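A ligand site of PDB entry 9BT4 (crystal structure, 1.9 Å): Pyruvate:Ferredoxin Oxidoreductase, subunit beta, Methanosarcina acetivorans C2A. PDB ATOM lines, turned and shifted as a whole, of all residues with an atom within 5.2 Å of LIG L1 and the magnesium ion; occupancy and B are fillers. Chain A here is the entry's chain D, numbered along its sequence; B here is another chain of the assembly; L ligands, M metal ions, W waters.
Residues that only touch LIG L1: Glu 68, Pro 36 of chain B, Tyr 129, Thr 132, Gln 91 of chain B, Gly 97, Phe 67 of chain A, Thr 43, Ile 37 of chain B, Ile 104, Tyr 35 of chain B, Gly 44 and Leu 95 of chain B.
The nearest printed residue that does not touch LIG L1 is Gly 92 of chain B (4.3 Å).
The backbone NH (N) of Asp 98 lies within hydrogen-bond range of the backbone carbonyl oxygen (O) of Val 124 (3.2 Å).
The backbone NH of Phe 67 of chain A is in hydrogen-bond range of the side-chain hydroxyl of Thr 43 (3.3 Å).
N of Asn 131 lies close to SG of Cys 45.
OG of Ser 100 lies within hydrogen-bond range of O of Phe 67 of chain A.
The backbone carbonyl oxygen of Gly 99 sits at hydrogen-bond distance from the backbone NH of Ile 104 (3.1 Å).
OD1 of Asp 22 lies within hydrogen-bond range of ND2 of Asn 126 (3.3 Å).
The backbone NH of Leu 46 lies within hydrogen-bond range of the side-chain carboxylate of Asp 22 (3.4 Å).
The side-chain hydroxyl (OH) of Tyr 129 lies within hydrogen-bond range of the side-chain hydroxyl (OH) of Tyr 35 of chain B (2.8 Å).
An oxygen (O6) of LIG L1 sits close to the side-chain carboxylate (OD2) of Asp 22, at 2.6 Å.
OE1 of Glu 67 of chain B sits at hydrogen-bond distance from N1 of LIG L1 (2.7 Å).
The backbone NH of Asp 98 sits close to an oxygen (O3) of LIG L1.
An oxygen (O7) of LIG L1 lies close to the backbone NH (N) of Met 130 (3.0 Å).
An iron atom (FE3) of LG2 L2 is bound by the side-chain sulfur of Cys 45, at 2.3 Å.
A sulfur (S1) of LG2 L2 lies close to the side-chain amide nitrogen (ND2) of Asn 126 (3.6 Å).
The backbone NH of Ser 100 lies within hydrogen-bond range of an oxygen (O2) of LIG L1 (2.9 Å).
An oxygen (O5) of LIG L1 lies within hydrogen-bond range of the backbone NH (N) of Asn 131 (3.0 Å).
The backbone NH (N) of Cys 45 sits at hydrogen-bond distance from an oxygen (O5) of LIG L1.
An oxygen (O2) of LIG L1 lies within hydrogen-bond range of the backbone NH (N) of Gly 99 (3.4 Å).
An oxygen (O5) of LIG L1 lies close to the side-chain sulfur (SG) of Cys 45 (3.7 Å).
Water W5 lies within hydrogen-bond range of the backbone carbonyl oxygen (O) of Val 124 (2.7 Å), an oxygen (O6) of LIG L1 (2.8 Å) and the side-chain amide nitrogen (ND2) of Asn 126 (3.1 Å).
Water W1 lies within hydrogen-bond range of O6 of LIG L1 (2.8 Å) and OD2 of Asp 22 (3.4 Å).
Water W4 lies within hydrogen-bond range of the backbone carbonyl oxygen of Thr 43 (2.6 Å), an oxygen (O2) of LIG L1 (2.8 Å) and the backbone NH of Gly 97 (3.0 Å).
Water W3 bridges NH2 of Arg 117 of chain B (2.8 Å) and N3 of LIG L1 (2.9 Å).
Water W2 lies within hydrogen-bond range of the side-chain hydroxyl of Thr 43 (2.7 Å) and a nitrogen (N3) of LIG L1 (3.4 Å).
The magnesium ion is bound by the backbone carbonyl oxygen of Ala 128 (2.0 Å), the side-chain amide oxygen of Asn 126 (2.0 Å), the side-chain carboxylate of Asp 98 (2.0 Å), an oxygen (O3) of LIG L1 (2.0 Å), an oxygen (O7) of LIG L1 (2.0 Å) and water W5 (2.4 Å).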
ATOM      1  N   ASP A  22       4.101 -27.848   7.582  1.00  0.00           N
ATOM      2  CA  ASP A  22       4.130 -26.757   8.546  1.00  0.00           C
ATOM      3  C   ASP A  22       4.736 -27.240   9.864  1.00  0.00           C
ATOM      4  O   ASP A  22       5.502 -26.502  10.488  1.00  0.00           O
ATOM      5  CB  ASP A  22       2.770 -26.120   8.749  1.00  0.00           C
ATOM      6  CG  ASP A  22       2.303 -25.146   7.673  1.00  0.00           C
ATOM      7  OD1 ASP A  22       2.901 -25.142   6.576  1.00  0.00           O
ATOM      8  OD2 ASP A  22       1.356 -24.383   7.950  1.00  0.00           O
ATOM      9  N   THR A  43      -2.164 -16.239  11.833  1.00  0.00           N
ATOM     10  CA  THR A  43      -3.187 -17.232  11.541  1.00  0.00           C
ATOM     11  C   THR A  43      -2.758 -18.097  10.359  1.00  0.00           C
ATOM     12  O   THR A  43      -2.220 -17.603   9.370  1.00  0.00           O
ATOM     13  CB  THR A  43      -4.518 -16.537  11.251  1.00  0.00           C
ATOM     14  OG1 THR A  43      -4.703 -15.515  12.225  1.00  0.00           O
ATOM     15  CG2 THR A  43      -5.699 -17.496  11.286  1.00  0.00           C
ATOM     16  N   GLY A  44      -3.051 -19.396  10.458  1.00  0.00           N
ATOM     17  CA  GLY A  44      -2.747 -20.349   9.407  1.00  0.00           C
ATOM     18  C   GLY A  44      -2.773 -21.758   9.969  1.00  0.00           C
ATOM     19  O   GLY A  44      -3.105 -21.936  11.140  1.00  0.00           O
ATOM     20  N   CYS A  45      -2.423 -22.742   9.143  1.00  0.00           N
ATOM     21  CA  CYS A  45      -2.447 -24.144   9.558  1.00  0.00           C
ATOM     22  C   CYS A  45      -1.596 -24.323  10.809  1.00  0.00           C
ATOM     23  O   CYS A  45      -2.038 -24.981  11.755  1.00  0.00           O
ATOM     24  CB  CYS A  45      -1.851 -25.018   8.470  1.00  0.00           C
ATOM     25  SG  CYS A  45      -3.045 -25.629   7.253  1.00  0.00           S
ATOM     26  N   LEU A  46      -0.380 -23.756  10.807  1.00  0.00           N
ATOM     27  CA  LEU A  46       0.552 -23.928  11.910  1.00  0.00           C
ATOM     28  C   LEU A  46      -0.105 -23.479  13.224  1.00  0.00           C
ATOM     29  O   LEU A  46      -0.092 -24.223  14.211  1.00  0.00           O
ATOM     30  CB  LEU A  46       1.856 -23.185  11.645  1.00  0.00           C
ATOM     31  CG  LEU A  46       2.882 -23.180  12.787  1.00  0.00           C
ATOM     32  CD1 LEU A  46       3.311 -24.598  13.155  1.00  0.00           C
ATOM     33  CD2 LEU A  46       4.088 -22.324  12.435  1.00  0.00           C
ATOM     34  N   PHE A  67      -4.064 -12.340  11.374  1.00  0.00           N
ATOM     35  CA  PHE A  67      -3.459 -12.900  10.168  1.00  0.00           C
ATOM     36  C   PHE A  67      -2.428 -11.933   9.586  1.00  0.00           C
ATOM     37  O   PHE A  67      -1.432 -12.369   9.020  1.00  0.00           O
ATOM     38  CB  PHE A  67      -4.610 -13.237   9.208  1.00  0.00           C
ATOM     39  CG  PHE A  67      -4.237 -14.007   7.936  1.00  0.00           C
ATOM     40  CD1 PHE A  67      -3.161 -14.896   7.919  1.00  0.00           C
ATOM     41  CD2 PHE A  67      -4.962 -13.829   6.764  1.00  0.00           C
ATOM     42  CE1 PHE A  67      -2.823 -15.572   6.758  1.00  0.00           C
ATOM     43  CE2 PHE A  67      -4.622 -14.528   5.602  1.00  0.00           C
ATOM     44  CZ  PHE A  67      -3.558 -15.387   5.604  1.00  0.00           C
ATOM     45  N   GLU A  68      -2.656 -10.625   9.770  1.00  0.00           N
ATOM     46  CA  GLU A  68      -1.931  -9.616   9.011  1.00  0.00           C
ATOM     47  C   GLU A  68      -0.726  -9.044   9.771  1.00  0.00           C
ATOM     48  O   GLU A  68       0.093  -8.360   9.168  1.00  0.00           O
ATOM     49  CB  GLU A  68      -2.819  -8.428   8.619  1.00  0.00           C
ATOM     50  CG  GLU A  68      -4.250  -8.798   8.206  1.00  0.00           C
ATOM     51  CD  GLU A  68      -5.308  -8.744   9.298  1.00  0.00           C
ATOM     52  OE1 GLU A  68      -5.037  -9.210  10.419  1.00  0.00           O
ATOM     53  OE2 GLU A  68      -6.425  -8.254   9.029  1.00  0.00           O
ATOM     54  N   GLY A  96       5.301 -17.600   9.847  1.00  0.00           N
ATOM     55  CA  GLY A  96       4.030 -17.461   9.146  1.00  0.00           C
ATOM     56  C   GLY A  96       4.093 -18.118   7.776  1.00  0.00           C
ATOM     57  O   GLY A  96       5.161 -18.358   7.250  1.00  0.00           O
ATOM     58  N   GLY A  97       2.906 -18.391   7.217  1.00  0.00           N
ATOM     59  CA  GLY A  97       2.812 -18.981   5.892  1.00  0.00           C
ATOM     60  C   GLY A  97       3.043 -17.943   4.798  1.00  0.00           C
ATOM     61  O   GLY A  97       3.144 -16.740   5.065  1.00  0.00           O
ATOM     62  N   ASP A  98       3.095 -18.438   3.560  1.00  0.00           N
ATOM     63  CA  ASP A  98       3.245 -17.632   2.355  1.00  0.00           C
ATOM     64  C   ASP A  98       2.174 -16.543   2.321  1.00  0.00           C
ATOM     65  O   ASP A  98       2.464 -15.381   2.054  1.00  0.00           O
ATOM     66  CB  ASP A  98       3.270 -18.522   1.118  1.00  0.00           C
ATOM     67  CG  ASP A  98       2.150 -19.548   1.019  1.00  0.00           C
ATOM     68  OD1 ASP A  98       2.053 -20.432   1.907  1.00  0.00           O
ATOM     69  OD2 ASP A  98       1.354 -19.449   0.051  1.00  0.00           O
ATOM     70  N   GLY A  99       0.922 -16.931   2.592  1.00  0.00           N
ATOM     71  CA  GLY A  99      -0.201 -16.005   2.558  1.00  0.00           C
ATOM     72  C   GLY A  99      -0.035 -14.869   3.556  1.00  0.00           C
ATOM     73  O   GLY A  99      -0.194 -13.692   3.215  1.00  0.00           O
ATOM     74  N   SER A 100       0.312 -15.234   4.795  1.00  0.00           N
ATOM     75  CA  SER A 100       0.509 -14.253   5.856  1.00  0.00           C
ATOM     76  C   SER A 100       1.691 -13.329   5.561  1.00  0.00           C
ATOM     77  O   SER A 100       1.634 -12.140   5.868  1.00  0.00           O
ATOM     78  CB  SER A 100       0.674 -14.929   7.199  1.00  0.00           C
ATOM     79  OG  SER A 100       0.588 -13.952   8.217  1.00  0.00           O
ATOM     80  N   ILE A 104      -1.039 -10.678   2.915  1.00  0.00           N
ATOM     81  CA  ILE A 104      -1.833  -9.839   3.798  1.00  0.00           C
ATOM     82  C   ILE A 104      -0.944  -9.187   4.862  1.00  0.00           C
ATOM     83  O   ILE A 104      -1.310  -8.168   5.439  1.00  0.00           O
ATOM     84  CB  ILE A 104      -3.027 -10.609   4.374  1.00  0.00           C
ATOM     85  CG1 ILE A 104      -4.157  -9.676   4.802  1.00  0.00           C
ATOM     86  CG2 ILE A 104      -2.610 -11.567   5.498  1.00  0.00           C
ATOM     87  CD1 ILE A 104      -5.476 -10.368   5.086  1.00  0.00           C
ATOM     88  N   VAL A 124       6.947 -19.893   5.936  1.00  0.00           N
ATOM     89  CA  VAL A 124       6.693 -21.287   5.615  1.00  0.00           C
ATOM     90  C   VAL A 124       5.864 -21.321   4.333  1.00  0.00           C
ATOM     91  O   VAL A 124       4.640 -21.165   4.378  1.00  0.00           O
ATOM     92  CB  VAL A 124       6.000 -22.036   6.770  1.00  0.00           C
ATOM     93  CG1 VAL A 124       5.807 -23.518   6.458  1.00  0.00           C
ATOM     94  CG2 VAL A 124       6.745 -21.873   8.089  1.00  0.00           C
ATOM     95  N   ASN A 126       4.132 -22.925   1.472  1.00  0.00           N
ATOM     96  CA  ASN A 126       3.497 -24.099   0.880  1.00  0.00           C
ATOM     97  C   ASN A 126       2.676 -23.719  -0.356  1.00  0.00           C
ATOM     98  O   ASN A 126       1.865 -24.515  -0.808  1.00  0.00           O
ATOM     99  CB  ASN A 126       2.767 -24.922   1.937  1.00  0.00           C
ATOM    100  CG  ASN A 126       1.659 -24.149   2.630  1.00  0.00           C
ATOM    101  OD1 ASN A 126       1.168 -23.140   2.125  1.00  0.00           O
ATOM    102  ND2 ASN A 126       1.250 -24.642   3.795  1.00  0.00           N
ATOM    103  N   GLU A 127       2.865 -22.495  -0.863  1.00  0.00           N
ATOM    104  CA  GLU A 127       2.438 -22.082  -2.192  1.00  0.00           C
ATOM    105  C   GLU A 127       0.917 -22.063  -2.348  1.00  0.00           C
ATOM    106  O   GLU A 127       0.399 -22.187  -3.464  1.00  0.00           O
ATOM    107  CB  GLU A 127       3.134 -22.942  -3.254  1.00  0.00           C
ATOM    108  CG  GLU A 127       4.643 -22.735  -3.250  1.00  0.00           C
ATOM    109  CD  GLU A 127       5.416 -23.341  -4.411  1.00  0.00           C
ATOM    110  OE1 GLU A 127       4.886 -24.236  -5.104  1.00  0.00           O
ATOM    111  OE2 GLU A 127       6.565 -22.894  -4.623  1.00  0.00           O
ATOM    112  N   ALA A 128       0.199 -21.882  -1.227  1.00  0.00           N
ATOM    113  CA  ALA A 128      -1.230 -21.617  -1.201  1.00  0.00           C
ATOM    114  C   ALA A 128      -1.655 -21.289   0.238  1.00  0.00           C
ATOM    115  O   ALA A 128      -0.866 -21.424   1.179  1.00  0.00           O
ATOM    116  CB  ALA A 128      -2.004 -22.794  -1.759  1.00  0.00           C
ATOM    117  N   TYR A 129      -2.901 -20.822   0.356  1.00  0.00           N
ATOM    118  CA  TYR A 129      -3.566 -20.675   1.648  1.00  0.00           C
ATOM    119  C   TYR A 129      -4.172 -22.027   2.005  1.00  0.00           C
ATOM    120  O   TYR A 129      -5.215 -22.406   1.464  1.00  0.00           O
ATOM    121  CB  TYR A 129      -4.702 -19.642   1.585  1.00  0.00           C
ATOM    122  CG  TYR A 129      -4.326 -18.212   1.223  1.00  0.00           C
ATOM    123  CD1 TYR A 129      -3.667 -17.379   2.123  1.00  0.00           C
ATOM    124  CD2 TYR A 129      -4.681 -17.676  -0.009  1.00  0.00           C
ATOM    125  CE1 TYR A 129      -3.356 -16.073   1.799  1.00  0.00           C
ATOM    126  CE2 TYR A 129      -4.371 -16.366  -0.346  1.00  0.00           C
ATOM    127  CZ  TYR A 129      -3.689 -15.567   0.547  1.00  0.00           C
ATOM    128  OH  TYR A 129      -3.385 -14.284   0.223  1.00  0.00           O
ATOM    129  N   MET A 130      -3.528 -22.762   2.923  1.00  0.00           N
ATOM    130  CA  MET A 130      -3.895 -24.149   3.164  1.00  0.00           C
ATOM    131  C   MET A 130      -5.019 -24.259   4.189  1.00  0.00           C
ATOM    132  O   MET A 130      -5.951 -25.032   3.981  1.00  0.00           O
ATOM    133  CB  MET A 130      -2.700 -25.019   3.548  1.00  0.00           C
ATOM    134  CG  MET A 130      -1.709 -25.215   2.413  1.00  0.00           C
ATOM    135  SD  MET A 130      -2.506 -25.576   0.833  1.00  0.00           S
ATOM    136  CE  MET A 130      -1.057 -25.935  -0.167  1.00  0.00           C
ATOM    137  N   ASN A 131      -4.935 -23.507   5.293  1.00  0.00           N
ATOM    138  CA  ASN A 131      -5.896 -23.690   6.377  1.00  0.00           C
ATOM    139  C   ASN A 131      -7.327 -23.473   5.860  1.00  0.00           C
ATOM    140  O   ASN A 131      -8.247 -24.138   6.321  1.00  0.00           O
ATOM    141  CB  ASN A 131      -5.621 -22.798   7.580  1.00  0.00           C
ATOM    142  CG  ASN A 131      -6.417 -23.235   8.785  1.00  0.00           C
ATOM    143  OD1 ASN A 131      -6.148 -24.297   9.360  1.00  0.00           O
ATOM    144  ND2 ASN A 131      -7.392 -22.433   9.198  1.00  0.00           N
ATOM    145  N   THR A 132      -7.479 -22.556   4.901  1.00  0.00           N
ATOM    146  CA  THR A 132      -8.779 -22.171   4.372  1.00  0.00           C
ATOM    147  C   THR A 132      -9.240 -23.081   3.232  1.00  0.00           C
ATOM    148  O   THR A 132     -10.383 -22.973   2.801  1.00  0.00           O
ATOM    149  CB  THR A 132      -8.784 -20.692   3.964  1.00  0.00           C
ATOM    150  OG1 THR A 132      -7.544 -20.456   3.310  1.00  0.00           O
ATOM    151  CG2 THR A 132      -8.985 -19.780   5.157  1.00  0.00           C
ATOM    152  N   TYR B  35     -11.156 -12.658  -1.564  1.00  0.00           N
ATOM    153  CA  TYR B  35     -10.135 -13.056  -0.608  1.00  0.00           C
ATOM    154  C   TYR B  35     -10.690 -14.192   0.233  1.00  0.00           C
ATOM    155  O   TYR B  35     -11.812 -14.102   0.742  1.00  0.00           O
ATOM    156  CB  TYR B  35      -9.601 -11.866   0.210  1.00  0.00           C
ATOM    157  CG  TYR B  35      -8.260 -12.204   0.850  1.00  0.00           C
ATOM    158  CD1 TYR B  35      -7.094 -12.171   0.094  1.00  0.00           C
ATOM    159  CD2 TYR B  35      -8.160 -12.580   2.183  1.00  0.00           C
ATOM    160  CE1 TYR B  35      -5.870 -12.502   0.642  1.00  0.00           C
ATOM    161  CE2 TYR B  35      -6.936 -12.902   2.749  1.00  0.00           C
ATOM    162  CZ  TYR B  35      -5.790 -12.872   1.971  1.00  0.00           C
ATOM    163  OH  TYR B  35      -4.570 -13.175   2.506  1.00  0.00           O
ATOM    164  N   PRO B  36      -9.961 -15.325   0.388  1.00  0.00           N
ATOM    165  CA  PRO B  36     -10.499 -16.489   1.099  1.00  0.00           C
ATOM    166  C   PRO B  36     -10.520 -16.324   2.616  1.00  0.00           C
ATOM    167  O   PRO B  36      -9.619 -15.733   3.199  1.00  0.00           O
ATOM    168  CB  PRO B  36      -9.550 -17.625   0.646  1.00  0.00           C
ATOM    169  CG  PRO B  36      -8.229 -16.926   0.424  1.00  0.00           C
ATOM    170  CD  PRO B  36      -8.592 -15.542  -0.105  1.00  0.00           C
ATOM    171  N   ILE B  37     -11.587 -16.860   3.225  1.00  0.00           N
ATOM    172  CA  ILE B  37     -11.720 -16.990   4.672  1.00  0.00           C
ATOM    173  C   ILE B  37     -12.877 -17.943   4.971  1.00  0.00           C
ATOM    174  O   ILE B  37     -13.973 -17.757   4.459  1.00  0.00           O
ATOM    175  CB  ILE B  37     -11.907 -15.621   5.370  1.00  0.00           C
ATOM    176  CG1 ILE B  37     -12.175 -15.776   6.873  1.00  0.00           C
ATOM    177  CG2 ILE B  37     -12.984 -14.776   4.687  1.00  0.00           C
ATOM    178  CD1 ILE B  37     -12.119 -14.468   7.656  1.00  0.00           C
ATOM    179  N   THR B  38     -12.600 -18.960   5.801  1.00  0.00           N
ATOM    180  CA  THR B  38     -13.609 -19.905   6.262  1.00  0.00           C
ATOM    181  C   THR B  38     -14.673 -19.134   7.033  1.00  0.00           C
ATOM    182  O   THR B  38     -14.340 -18.300   7.865  1.00  0.00           O
ATOM    183  CB  THR B  38     -12.934 -20.929   7.174  1.00  0.00           C
ATOM    184  OG1 THR B  38     -11.804 -21.443   6.479  1.00  0.00           O
ATOM    185  CG2 THR B  38     -13.854 -22.061   7.591  1.00  0.00           C
ATOM    186  N   GLU B  67      -8.562  -8.469   2.301  1.00  0.00           N
ATOM    187  CA  GLU B  67      -9.954  -8.036   2.225  1.00  0.00           C
ATOM    188  C   GLU B  67     -10.023  -6.523   2.022  1.00  0.00           C
ATOM    189  O   GLU B  67     -10.948  -6.031   1.376  1.00  0.00           O
ATOM    190  CB  GLU B  67     -10.781  -8.356   3.473  1.00  0.00           C
ATOM    191  CG  GLU B  67     -11.285  -9.798   3.474  1.00  0.00           C
ATOM    192  CD  GLU B  67     -10.345 -10.809   4.081  1.00  0.00           C
ATOM    193  OE1 GLU B  67      -9.205 -10.457   4.469  1.00  0.00           O
ATOM    194  OE2 GLU B  67     -10.783 -11.976   4.195  1.00  0.00           O
ATOM    195  N   GLN B  91     -13.170 -11.999  10.386  1.00  0.00           N
ATOM    196  CA  GLN B  91     -11.958 -11.212  10.400  1.00  0.00           C
ATOM    197  C   GLN B  91     -11.855 -10.378   9.126  1.00  0.00           C
ATOM    198  O   GLN B  91     -11.375  -9.246   9.162  1.00  0.00           O
ATOM    199  CB  GLN B  91     -10.698 -12.074  10.504  1.00  0.00           C
ATOM    200  CG  GLN B  91     -10.654 -12.977  11.734  1.00  0.00           C
ATOM    201  CD  GLN B  91     -10.949 -12.262  13.032  1.00  0.00           C
ATOM    202  OE1 GLN B  91     -10.432 -11.167  13.307  1.00  0.00           O
ATOM    203  NE2 GLN B  91     -11.798 -12.850  13.843  1.00  0.00           N
ATOM    204  N   GLY B  92     -12.332 -10.952   8.015  1.00  0.00           N
ATOM    205  CA  GLY B  92     -12.271 -10.289   6.722  1.00  0.00           C
ATOM    206  C   GLY B  92     -13.138  -9.030   6.706  1.00  0.00           C
ATOM    207  O   GLY B  92     -12.696  -7.968   6.255  1.00  0.00           O
ATOM    208  N   LEU B  95     -11.684  -6.241   8.901  1.00  0.00           N
ATOM    209  CA  LEU B  95     -10.587  -5.526   8.261  1.00  0.00           C
ATOM    210  C   LEU B  95     -11.149  -4.461   7.308  1.00  0.00           C
ATOM    211  O   LEU B  95     -10.590  -3.380   7.192  1.00  0.00           O
ATOM    212  CB  LEU B  95      -9.648  -6.506   7.556  1.00  0.00           C
ATOM    213  CG  LEU B  95      -8.532  -5.901   6.682  1.00  0.00           C
ATOM    214  CD1 LEU B  95      -7.603  -4.996   7.492  1.00  0.00           C
ATOM    215  CD2 LEU B  95      -7.724  -6.975   5.955  1.00  0.00           C
ATOM    216  N   ARG B 117     -19.612 -15.320  10.744  1.00  0.00           N
ATOM    217  CA  ARG B 117     -18.736 -16.096  11.603  1.00  0.00           C
ATOM    218  C   ARG B 117     -18.221 -15.216  12.736  1.00  0.00           C
ATOM    219  O   ARG B 117     -18.051 -14.015  12.583  1.00  0.00           O
ATOM    220  CB  ARG B 117     -17.608 -16.733  10.790  1.00  0.00           C
ATOM    221  CG  ARG B 117     -16.391 -17.142  11.620  1.00  0.00           C
ATOM    222  CD  ARG B 117     -15.149 -17.383  10.762  1.00  0.00           C
ATOM    223  NE  ARG B 117     -13.939 -17.125  11.538  1.00  0.00           N
ATOM    224  CZ  ARG B 117     -12.678 -17.161  11.103  1.00  0.00           C
ATOM    225  NH1 ARG B 117     -12.405 -17.479   9.848  1.00  0.00           N
ATOM    226  NH2 ARG B 117     -11.687 -16.894  11.941  1.00  0.00           N
ATOM    227  N   ILE B 123      -9.792 -16.611  18.415  1.00  0.00           N
ATOM    228  CA  ILE B 123     -10.185 -16.964  17.065  1.00  0.00           C
ATOM    229  C   ILE B 123     -11.103 -18.192  17.118  1.00  0.00           C
ATOM    230  O   ILE B 123     -10.942 -19.056  17.974  1.00  0.00           O
ATOM    231  CB  ILE B 123      -8.938 -17.177  16.171  1.00  0.00           C
ATOM    232  CG1 ILE B 123      -9.330 -17.419  14.701  1.00  0.00           C
ATOM    233  CG2 ILE B 123      -8.031 -18.276  16.720  1.00  0.00           C
ATOM    234  CD1 ILE B 123      -8.178 -17.272  13.724  1.00  0.00           C
HETATM  235  N1  LIG L   1      -8.457 -12.377   6.219  1.00  0.00           N
HETATM  236  C1  LIG L   1      -8.184 -11.986   7.473  1.00  0.00           C
HETATM  237  C2  LIG L   1      -8.053 -10.518   7.725  1.00  0.00           C
HETATM  238  N2  LIG L   1      -8.019 -12.808   8.509  1.00  0.00           N
HETATM  239  C3  LIG L   1      -8.155 -14.132   8.278  1.00  0.00           C
HETATM  240  N3  LIG L   1      -7.989 -14.941   9.341  1.00  0.00           N
HETATM  241  C4  LIG L   1      -8.417 -14.638   6.990  1.00  0.00           C
HETATM  242  C5  LIG L   1      -8.583 -13.696   5.996  1.00  0.00           C
HETATM  243  C6  LIG L   1      -8.591 -16.105   6.682  1.00  0.00           C
HETATM  244  N4  LIG L   1      -7.386 -16.928   6.789  1.00  0.00           N
HETATM  245  C7  LIG L   1      -6.917 -17.418   7.966  1.00  0.00           C
HETATM  246  S1  LIG L   1      -5.574 -18.376   7.706  1.00  0.00           S
HETATM  247  C8  LIG L   1      -5.599 -18.209   6.030  1.00  0.00           C
HETATM  248  C9  LIG L   1      -6.656 -17.396   5.673  1.00  0.00           C
HETATM  249  C10 LIG L   1      -7.012 -17.023   4.264  1.00  0.00           C
HETATM  250  C11 LIG L   1      -4.634 -18.876   5.131  1.00  0.00           C
HETATM  251  C12 LIG L   1      -3.261 -18.997   5.701  1.00  0.00           C
HETATM  252  O1  LIG L   1      -2.403 -19.261   4.576  1.00  0.00           O
HETATM  253  P1  LIG L   1      -0.817 -19.198   4.792  1.00  0.00           P
HETATM  254  O2  LIG L   1      -0.497 -17.936   5.520  1.00  0.00           O
HETATM  255  O3  LIG L   1      -0.136 -19.573   3.510  1.00  0.00           O
HETATM  256  O4  LIG L   1      -0.658 -20.412   5.828  1.00  0.00           O
HETATM  257  P2  LIG L   1      -0.939 -21.974   5.609  1.00  0.00           P
HETATM  258  O5  LIG L   1      -2.323 -22.219   6.167  1.00  0.00           O
HETATM  259  O6  LIG L   1       0.154 -22.652   6.378  1.00  0.00           O
HETATM  260  O7  LIG L   1      -0.824 -22.168   4.095  1.00  0.00           O
HETATM  261 FE1  LG2 L   2      -2.347 -30.257   6.274  1.00  0.00          FE
HETATM  262 FE2  LG2 L   2      -0.026 -29.236   7.186  1.00  0.00          FE
HETATM  263 FE3  LG2 L   2      -2.112 -27.550   6.543  1.00  0.00          FE
HETATM  264 FE4  LG2 L   2      -0.690 -28.841   4.558  1.00  0.00          FE
HETATM  265  S1  LG2 L   2       0.095 -27.263   6.000  1.00  0.00           S
HETATM  266  S2  LG2 L   2      -2.976 -28.662   4.768  1.00  0.00           S
HETATM  267  S3  LG2 L   2      -0.246 -30.803   5.585  1.00  0.00           S
HETATM  268  S4  LG2 L   2      -2.062 -29.109   8.219  1.00  0.00           S
HETATM  269 MG    MG M   1       0.434 -21.352   2.710  1.00  0.00          MG
HETATM  270  O   HOH W   1       0.754 -21.047   8.583  1.00  0.00           O
HETATM  271  O   HOH W   2      -7.005 -14.075  12.508  1.00  0.00           O
HETATM  272  O   HOH W   3      -9.560 -17.219  10.094  1.00  0.00           O
HETATM  273  O   HOH W   4       0.099 -18.138   8.244  1.00  0.00           O
HETATM  274  O   HOH W   5       1.991 -21.735   4.525  1.00  0.00           O
